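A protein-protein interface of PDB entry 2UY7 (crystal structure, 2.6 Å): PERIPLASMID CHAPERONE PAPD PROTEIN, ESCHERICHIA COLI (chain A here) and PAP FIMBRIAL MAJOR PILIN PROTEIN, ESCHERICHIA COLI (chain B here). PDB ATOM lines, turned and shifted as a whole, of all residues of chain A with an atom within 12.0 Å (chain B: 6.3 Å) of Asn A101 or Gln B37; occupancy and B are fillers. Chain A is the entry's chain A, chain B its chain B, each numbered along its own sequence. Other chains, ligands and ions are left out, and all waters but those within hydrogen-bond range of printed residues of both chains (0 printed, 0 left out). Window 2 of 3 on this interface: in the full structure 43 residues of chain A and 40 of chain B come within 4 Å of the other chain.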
ATOM      1  N   PRO A  95      25.783   0.243  -8.819  1.00  0.00           N
ATOM      2  CA  PRO A  95      26.118   1.660  -8.683  1.00  0.00           C
ATOM      3  C   PRO A  95      26.003   2.352 -10.041  1.00  0.00           C
ATOM      4  O   PRO A  95      26.143   1.707 -11.079  1.00  0.00           O
ATOM      5  CB  PRO A  95      27.556   1.618  -8.171  1.00  0.00           C
ATOM      6  CG  PRO A  95      28.105   0.381  -8.840  1.00  0.00           C
ATOM      7  CD  PRO A  95      26.976  -0.609  -8.653  1.00  0.00           C
ATOM      8  N   ARG A  96      25.739   3.655 -10.024  1.00  0.00           N
ATOM      9  CA  ARG A  96      25.628   4.433 -11.255  1.00  0.00           C
ATOM     10  C   ARG A  96      26.947   4.315 -12.013  1.00  0.00           C
ATOM     11  O   ARG A  96      28.020   4.385 -11.411  1.00  0.00           O
ATOM     12  CB  ARG A  96      25.341   5.895 -10.930  1.00  0.00           C
ATOM     13  N   SER A  97      26.869   4.138 -13.329  1.00  0.00           N
ATOM     14  CA  SER A  97      28.072   4.001 -14.139  1.00  0.00           C
ATOM     15  C   SER A  97      28.835   5.308 -14.350  1.00  0.00           C
ATOM     16  O   SER A  97      28.248   6.379 -14.516  1.00  0.00           O
ATOM     17  CB  SER A  97      27.726   3.399 -15.501  1.00  0.00           C
ATOM     18  OG  SER A  97      28.907   3.129 -16.238  1.00  0.00           O
ATOM     19  N   GLU A  98      30.158   5.196 -14.341  1.00  0.00           N
ATOM     20  CA  GLU A  98      31.033   6.339 -14.558  1.00  0.00           C
ATOM     21  C   GLU A  98      30.972   6.732 -16.047  1.00  0.00           C
ATOM     22  O   GLU A  98      30.967   7.915 -16.381  1.00  0.00           O
ATOM     23  CB  GLU A  98      32.471   5.964 -14.185  1.00  0.00           C
ATOM     24  CG  GLU A  98      33.245   7.060 -13.479  1.00  0.00           C
ATOM     25  CD  GLU A  98      32.784   7.261 -12.043  1.00  0.00           C
ATOM     26  OE1 GLU A  98      32.999   6.345 -11.213  1.00  0.00           O
ATOM     27  OE2 GLU A  98      32.205   8.332 -11.746  1.00  0.00           O
ATOM     28  N   LYS A  99      30.916   5.725 -16.924  1.00  0.00           N
ATOM     29  CA  LYS A  99      30.864   5.923 -18.373  1.00  0.00           C
ATOM     30  C   LYS A  99      29.561   6.577 -18.862  1.00  0.00           C
ATOM     31  O   LYS A  99      28.534   6.517 -18.185  1.00  0.00           O
ATOM     32  CB  LYS A  99      31.081   4.585 -19.077  1.00  0.00           C
ATOM     33  N   ALA A 100      29.614   7.185 -20.049  1.00  0.00           N
ATOM     34  CA  ALA A 100      28.470   7.886 -20.637  1.00  0.00           C
ATOM     35  C   ALA A 100      27.368   7.017 -21.249  1.00  0.00           C
ATOM     36  O   ALA A 100      26.322   6.829 -20.636  1.00  0.00           O
ATOM     37  CB  ALA A 100      28.963   8.895 -21.672  1.00  0.00           C
ATOM     38  N   ASN A 101      27.594   6.503 -22.456  1.00  0.00           N
ATOM     39  CA  ASN A 101      26.606   5.675 -23.151  1.00  0.00           C
ATOM     40  C   ASN A 101      26.780   4.247 -22.712  1.00  0.00           C
ATOM     41  O   ASN A 101      27.669   3.556 -23.188  1.00  0.00           O
ATOM     42  CB  ASN A 101      26.827   5.777 -24.651  1.00  0.00           C
ATOM     43  CG  ASN A 101      27.100   7.189 -25.084  1.00  0.00           C
ATOM     44  OD1 ASN A 101      26.417   8.121 -24.653  1.00  0.00           O
ATOM     45  ND2 ASN A 101      28.105   7.365 -25.938  1.00  0.00           N
ATOM     46  N   VAL A 102      25.905   3.779 -21.835  1.00  0.00           N
ATOM     47  CA  VAL A 102      26.082   2.440 -21.318  1.00  0.00           C
ATOM     48  C   VAL A 102      24.814   1.650 -20.977  1.00  0.00           C
ATOM     49  O   VAL A 102      23.734   2.211 -20.794  1.00  0.00           O
ATOM     50  CB  VAL A 102      26.987   2.537 -20.078  1.00  0.00           C
ATOM     51  CG1 VAL A 102      26.217   3.174 -18.932  1.00  0.00           C
ATOM     52  CG2 VAL A 102      27.529   1.185 -19.722  1.00  0.00           C
ATOM     53  N   LEU A 103      24.974   0.333 -20.897  1.00  0.00           N
ATOM     54  CA  LEU A 103      23.898  -0.599 -20.562  1.00  0.00           C
ATOM     55  C   LEU A 103      24.357  -1.387 -19.328  1.00  0.00           C
ATOM     56  O   LEU A 103      25.433  -1.981 -19.351  1.00  0.00           O
ATOM     57  CB  LEU A 103      23.694  -1.577 -21.723  1.00  0.00           C
ATOM     58  CG  LEU A 103      22.506  -2.554 -21.776  1.00  0.00           C
ATOM     59  CD1 LEU A 103      23.007  -3.902 -22.280  1.00  0.00           C
ATOM     60  CD2 LEU A 103      21.857  -2.719 -20.425  1.00  0.00           C
ATOM     61  N   GLN A 104      23.565  -1.395 -18.259  1.00  0.00           N
ATOM     62  CA  GLN A 104      23.939  -2.152 -17.062  1.00  0.00           C
ATOM     63  C   GLN A 104      22.988  -3.299 -16.811  1.00  0.00           C
ATOM     64  O   GLN A 104      21.790  -3.200 -17.088  1.00  0.00           O
ATOM     65  CB  GLN A 104      23.953  -1.273 -15.812  1.00  0.00           C
ATOM     66  CG  GLN A 104      25.020  -0.214 -15.792  1.00  0.00           C
ATOM     67  CD  GLN A 104      25.068   0.508 -14.467  1.00  0.00           C
ATOM     68  OE1 GLN A 104      25.573  -0.027 -13.479  1.00  0.00           O
ATOM     69  NE2 GLN A 104      24.531   1.724 -14.431  1.00  0.00           N
ATOM     70  N   ILE A 105      23.534  -4.380 -16.269  1.00  0.00           N
ATOM     71  CA  ILE A 105      22.762  -5.569 -15.944  1.00  0.00           C
ATOM     72  C   ILE A 105      22.618  -5.654 -14.432  1.00  0.00           C
ATOM     73  O   ILE A 105      23.583  -5.413 -13.705  1.00  0.00           O
ATOM     74  CB  ILE A 105      23.484  -6.843 -16.433  1.00  0.00           C
ATOM     75  CG1 ILE A 105      23.558  -6.838 -17.959  1.00  0.00           C
ATOM     76  CG2 ILE A 105      22.781  -8.075 -15.919  1.00  0.00           C
ATOM     77  CD1 ILE A 105      22.215  -6.688 -18.627  1.00  0.00           C
ATOM     78  N   ILE B  33      28.333  -2.237 -20.168  1.00  0.00           N
ATOM     79  CA  ILE B  33      29.052  -2.350 -21.434  1.00  0.00           C
ATOM     80  C   ILE B  33      28.998  -0.950 -22.025  1.00  0.00           C
ATOM     81  O   ILE B  33      27.951  -0.310 -22.039  1.00  0.00           O
ATOM     82  CB  ILE B  33      28.434  -3.363 -22.425  1.00  0.00           C
ATOM     83  CG1 ILE B  33      26.962  -3.056 -22.659  1.00  0.00           C
ATOM     84  CG2 ILE B  33      28.682  -4.783 -21.929  1.00  0.00           C
ATOM     85  CD1 ILE B  33      26.340  -3.954 -23.706  1.00  0.00           C
ATOM     86  N   ASP B  34      30.150  -0.471 -22.471  1.00  0.00           N
ATOM     87  CA  ASP B  34      30.275   0.871 -23.026  1.00  0.00           C
ATOM     88  C   ASP B  34      30.125   0.861 -24.544  1.00  0.00           C
ATOM     89  O   ASP B  34      30.857   0.156 -25.242  1.00  0.00           O
ATOM     90  CB  ASP B  34      31.642   1.436 -22.626  1.00  0.00           C
ATOM     91  CG  ASP B  34      31.790   2.902 -22.947  1.00  0.00           C
ATOM     92  OD1 ASP B  34      30.777   3.555 -23.289  1.00  0.00           O
ATOM     93  OD2 ASP B  34      32.929   3.404 -22.846  1.00  0.00           O
ATOM     94  N   PHE B  35      29.175   1.639 -25.052  1.00  0.00           N
ATOM     95  CA  PHE B  35      28.959   1.696 -26.494  1.00  0.00           C
ATOM     96  C   PHE B  35      29.837   2.743 -27.164  1.00  0.00           C
ATOM     97  O   PHE B  35      29.959   2.771 -28.389  1.00  0.00           O
ATOM     98  CB  PHE B  35      27.495   1.992 -26.808  1.00  0.00           C
ATOM     99  CG  PHE B  35      26.557   0.888 -26.430  1.00  0.00           C
ATOM    100  CD1 PHE B  35      25.803   0.966 -25.265  1.00  0.00           C
ATOM    101  CD2 PHE B  35      26.413  -0.228 -27.251  1.00  0.00           C
ATOM    102  CE1 PHE B  35      24.916  -0.049 -24.924  1.00  0.00           C
ATOM    103  CE2 PHE B  35      25.527  -1.255 -26.920  1.00  0.00           C
ATOM    104  CZ  PHE B  35      24.776  -1.165 -25.755  1.00  0.00           C
ATOM    105  N   GLY B  36      30.457   3.595 -26.355  1.00  0.00           N
ATOM    106  CA  GLY B  36      31.299   4.641 -26.898  1.00  0.00           C
ATOM    107  C   GLY B  36      30.438   5.704 -27.558  1.00  0.00           C
ATOM    108  O   GLY B  36      29.212   5.577 -27.600  1.00  0.00           O
ATOM    109  N   GLN B  37      31.069   6.757 -28.065  1.00  0.00           N
ATOM    110  CA  GLN B  37      30.326   7.821 -28.724  1.00  0.00           C
ATOM    111  C   GLN B  37      29.748   7.294 -30.026  1.00  0.00           C
ATOM    112  O   GLN B  37      30.407   6.550 -30.749  1.00  0.00           O
ATOM    113  CB  GLN B  37      31.234   9.020 -28.996  1.00  0.00           C
ATOM    114  CG  GLN B  37      31.656   9.750 -27.735  1.00  0.00           C
ATOM    115  CD  GLN B  37      30.466  10.184 -26.895  1.00  0.00           C
ATOM    116  OE1 GLN B  37      29.693  11.049 -27.297  1.00  0.00           O
ATOM    117  NE2 GLN B  37      30.309   9.572 -25.726  1.00  0.00           N
ATOM    118  N   LEU B  38      28.505   7.668 -30.309  1.00  0.00           N
ATOM    119  CA  LEU B  38      27.849   7.224 -31.527  1.00  0.00           C
ATOM    120  C   LEU B  38      27.470   8.420 -32.386  1.00  0.00           C
ATOM    121  O   LEU B  38      27.275   9.522 -31.879  1.00  0.00           O
ATOM    122  CB  LEU B  38      26.605   6.410 -31.180  1.00  0.00           C
ATOM    123  CG  LEU B  38      26.836   5.170 -30.307  1.00  0.00           C
ATOM    124  CD1 LEU B  38      25.507   4.458 -30.076  1.00  0.00           C
ATOM    125  CD2 LEU B  38      27.839   4.229 -30.984  1.00  0.00           C
ATOM    126  N   SER B  39      27.374   8.206 -33.690  1.00  0.00           N
ATOM    127  CA  SER B  39      27.012   9.283 -34.605  1.00  0.00           C
ATOM    128  C   SER B  39      25.502   9.482 -34.679  1.00  0.00           C
ATOM    129  O   SER B  39      24.766   8.558 -35.030  1.00  0.00           O
ATOM    130  CB  SER B  39      27.555   8.983 -36.009  1.00  0.00           C
ATOM    131  OG  SER B  39      26.991   9.853 -36.981  1.00  0.00           O
ATOM    132  N   THR B  99      17.924  10.842 -25.571  1.00  0.00           N
ATOM    133  CA  THR B  99      18.615  10.806 -26.858  1.00  0.00           C
ATOM    134  C   THR B  99      17.817  10.227 -28.027  1.00  0.00           C
ATOM    135  O   THR B  99      18.212  10.398 -29.178  1.00  0.00           O
ATOM    136  CB  THR B  99      19.919  10.006 -26.770  1.00  0.00           C
ATOM    137  OG1 THR B  99      19.622   8.639 -26.454  1.00  0.00           O
ATOM    138  CG2 THR B  99      20.825  10.600 -25.709  1.00  0.00           C
ATOM    139  N   GLY B 150      23.918  13.405 -27.017  1.00  0.00           N
ATOM    140  CA  GLY B 150      23.964  13.318 -25.570  1.00  0.00           C
ATOM    141  C   GLY B 150      24.210  11.916 -25.054  1.00  0.00           C
ATOM    142  O   GLY B 150      24.085  10.934 -25.788  1.00  0.00           O
ATOM    143  N   ALA B 151      24.563  11.825 -23.777  1.00  0.00           N
ATOM    144  CA  ALA B 151      24.832  10.540 -23.149  1.00  0.00           C
ATOM    145  C   ALA B 151      23.529   9.839 -22.789  1.00  0.00           C
ATOM    146  O   ALA B 151      22.517  10.480 -22.506  1.00  0.00           O
ATOM    147  CB  ALA B 151      25.683  10.734 -21.901  1.00  0.00           C
ATOM    148  N   PHE B 152      23.565   8.516 -22.815  1.00  0.00           N
ATOM    149  CA  PHE B 152      22.396   7.720 -22.494  1.00  0.00           C
ATOM    150  C   PHE B 152      22.836   6.500 -21.702  1.00  0.00           C
ATOM    151  O   PHE B 152      24.019   6.171 -21.647  1.00  0.00           O
ATOM    152  CB  PHE B 152      21.689   7.283 -23.776  1.00  0.00           C
ATOM    153  CG  PHE B 152      22.508   6.369 -24.632  1.00  0.00           C
ATOM    154  CD1 PHE B 152      22.452   4.990 -24.450  1.00  0.00           C
ATOM    155  CD2 PHE B 152      23.353   6.885 -25.609  1.00  0.00           C
ATOM    156  CE1 PHE B 152      23.225   4.139 -25.233  1.00  0.00           C
ATOM    157  CE2 PHE B 152      24.131   6.048 -26.395  1.00  0.00           C
ATOM    158  CZ  PHE B 152      24.068   4.669 -26.209  1.00  0.00           C
ATOM    159  N   SER B 153      21.870   5.827 -21.099  1.00  0.00           N
ATOM    160  CA  SER B 153      22.140   4.650 -20.297  1.00  0.00           C
ATOM    161  C   SER B 153      20.839   3.901 -20.129  1.00  0.00           C
ATOM    162  O   SER B 153      19.759   4.460 -20.318  1.00  0.00           O
ATOM    163  CB  SER B 153      22.633   5.062 -18.923  1.00  0.00           C
ATOM    164  OG  SER B 153      21.606   5.755 -18.241  1.00  0.00           O
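O of Ala A100 sits close to O of Phe B152 (2.6 Å).
O of Asn A101 is in hydrogen-bond range of N of Phe B35 (3.1 Å).
O of Gly B36 lies within hydrogen-bond range of ND2 of Asn A101, at 2.7 Å.
The side-chain amide nitrogen (ND2) of Asn A101 sits close to the side-chain amide nitrogen (NE2) of Gln B37 (3.1 Å).
The side-chain amide oxygen (OD1) of Asn A101 is in hydrogen-bond range of the backbone NH (N) of Phe B152, at 3.4 Å.
O of Phe B152 lies within hydrogen-bond range of N of Val A102 (3.1 Å).
N of Ile B33 lies within hydrogen-bond range of O of Leu A103, at 3.0 Å.
The backbone carbonyl oxygen (O) of Asn A101 sits close to the side-chain carboxylate (OD1) of Asp B34 (3.1 Å).
The side-chain carboxylate of Asp B34 is in hydrogen-bond range of the backbone NH of Gly B36, 3.1 Å away.
Among the printed residues, merely in contact across the chains: Ala A100 with Ala B151 (3.8 Å), Asn A101 with Gly B150 (3.8 Å), Asn A101 with Ala B151 (3.3 Å), Val A102 with Ile B33 (2.8 Å), Val A102 with Ser B153 (3.0 Å) and Leu A103 with Phe B35 (3.8 Å).
Of the printed residues of chain B, Ala A100 touches Ala B151 (3.8 Å) and Phe B152 (2.6 Å).
Of chain B, only Asp B34, Phe B35, Gly B36, Gln B37, Gly B150, Ala B151 and Phe B152 come within 4 Å of Asn A101.
Of the printed residues of chain B, Val A102 touches Ile B33, Phe B152 and Ser B153.
Printed residues of chain B within 4 Å of Leu A103: Ile B33 (3.0 Å) and Phe B35 (3.8 Å).
Ile A105 touches none of the printed residues of chain B.
Printed residues of chain A within 4 Å of Ile B33: Val A102 and Leu A103.
Of the printed residues of chain A, Asp B34 touches Asn A101.
Phe B35 touches just these residues of chain A: Asn A101 (3.1 Å) and Leu A103 (3.8 Å).
Of chain A, only Asn A101 (2.7 Å) comes within 4 Å of Gly B36.
Gln B37 touches one residue of chain A.
No residue of chain A comes within 4 Å of Leu B38.
No residue of chain A comes within 4 Å of Ser B39.
Gly B150 touches just one residue of chain A: Asn A101 (3.8 Å).
Of the printed residues of chain A, Ala B151 touches Ala A100 (3.8 Å) and Asn A101 (3.3 Å).
Of chain A, only Ala A100 (2.6 Å), Asn A101 (3.0 Å) and Val A102 (3.1 Å) come within 4 Å of Phe B152.
Of chain A, only Val A102 (3.0 Å) comes within 4 Å of Ser B153.
The nearest residue of chain A that does not touch Gln B37 is Ala A100 (4.3 Å).
The nearest printed residue of chain A that does not touch Ile B33 is Asn A101 (4.04 Å).
Of the 12 printed residues of chain B, 9 touch a printed residue of chain A.
Hydrophobic or aromatic side chains of chain B that line the printed part of chain A: Ile B33, Phe B35, Ala B151 and Phe B152.
Of the 11 printed residues of chain A, 4 touch a printed residue of chain B.
Hydrophobic or aromatic side chains of chain A within 4 Å of the printed part of chain B: Ala A100, Val A102 and Leu A103.
Among the printed residues, no Asp or Glu carboxylate lies within 4 Å of a Lys or Arg side-chain nitrogen of the other chain.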
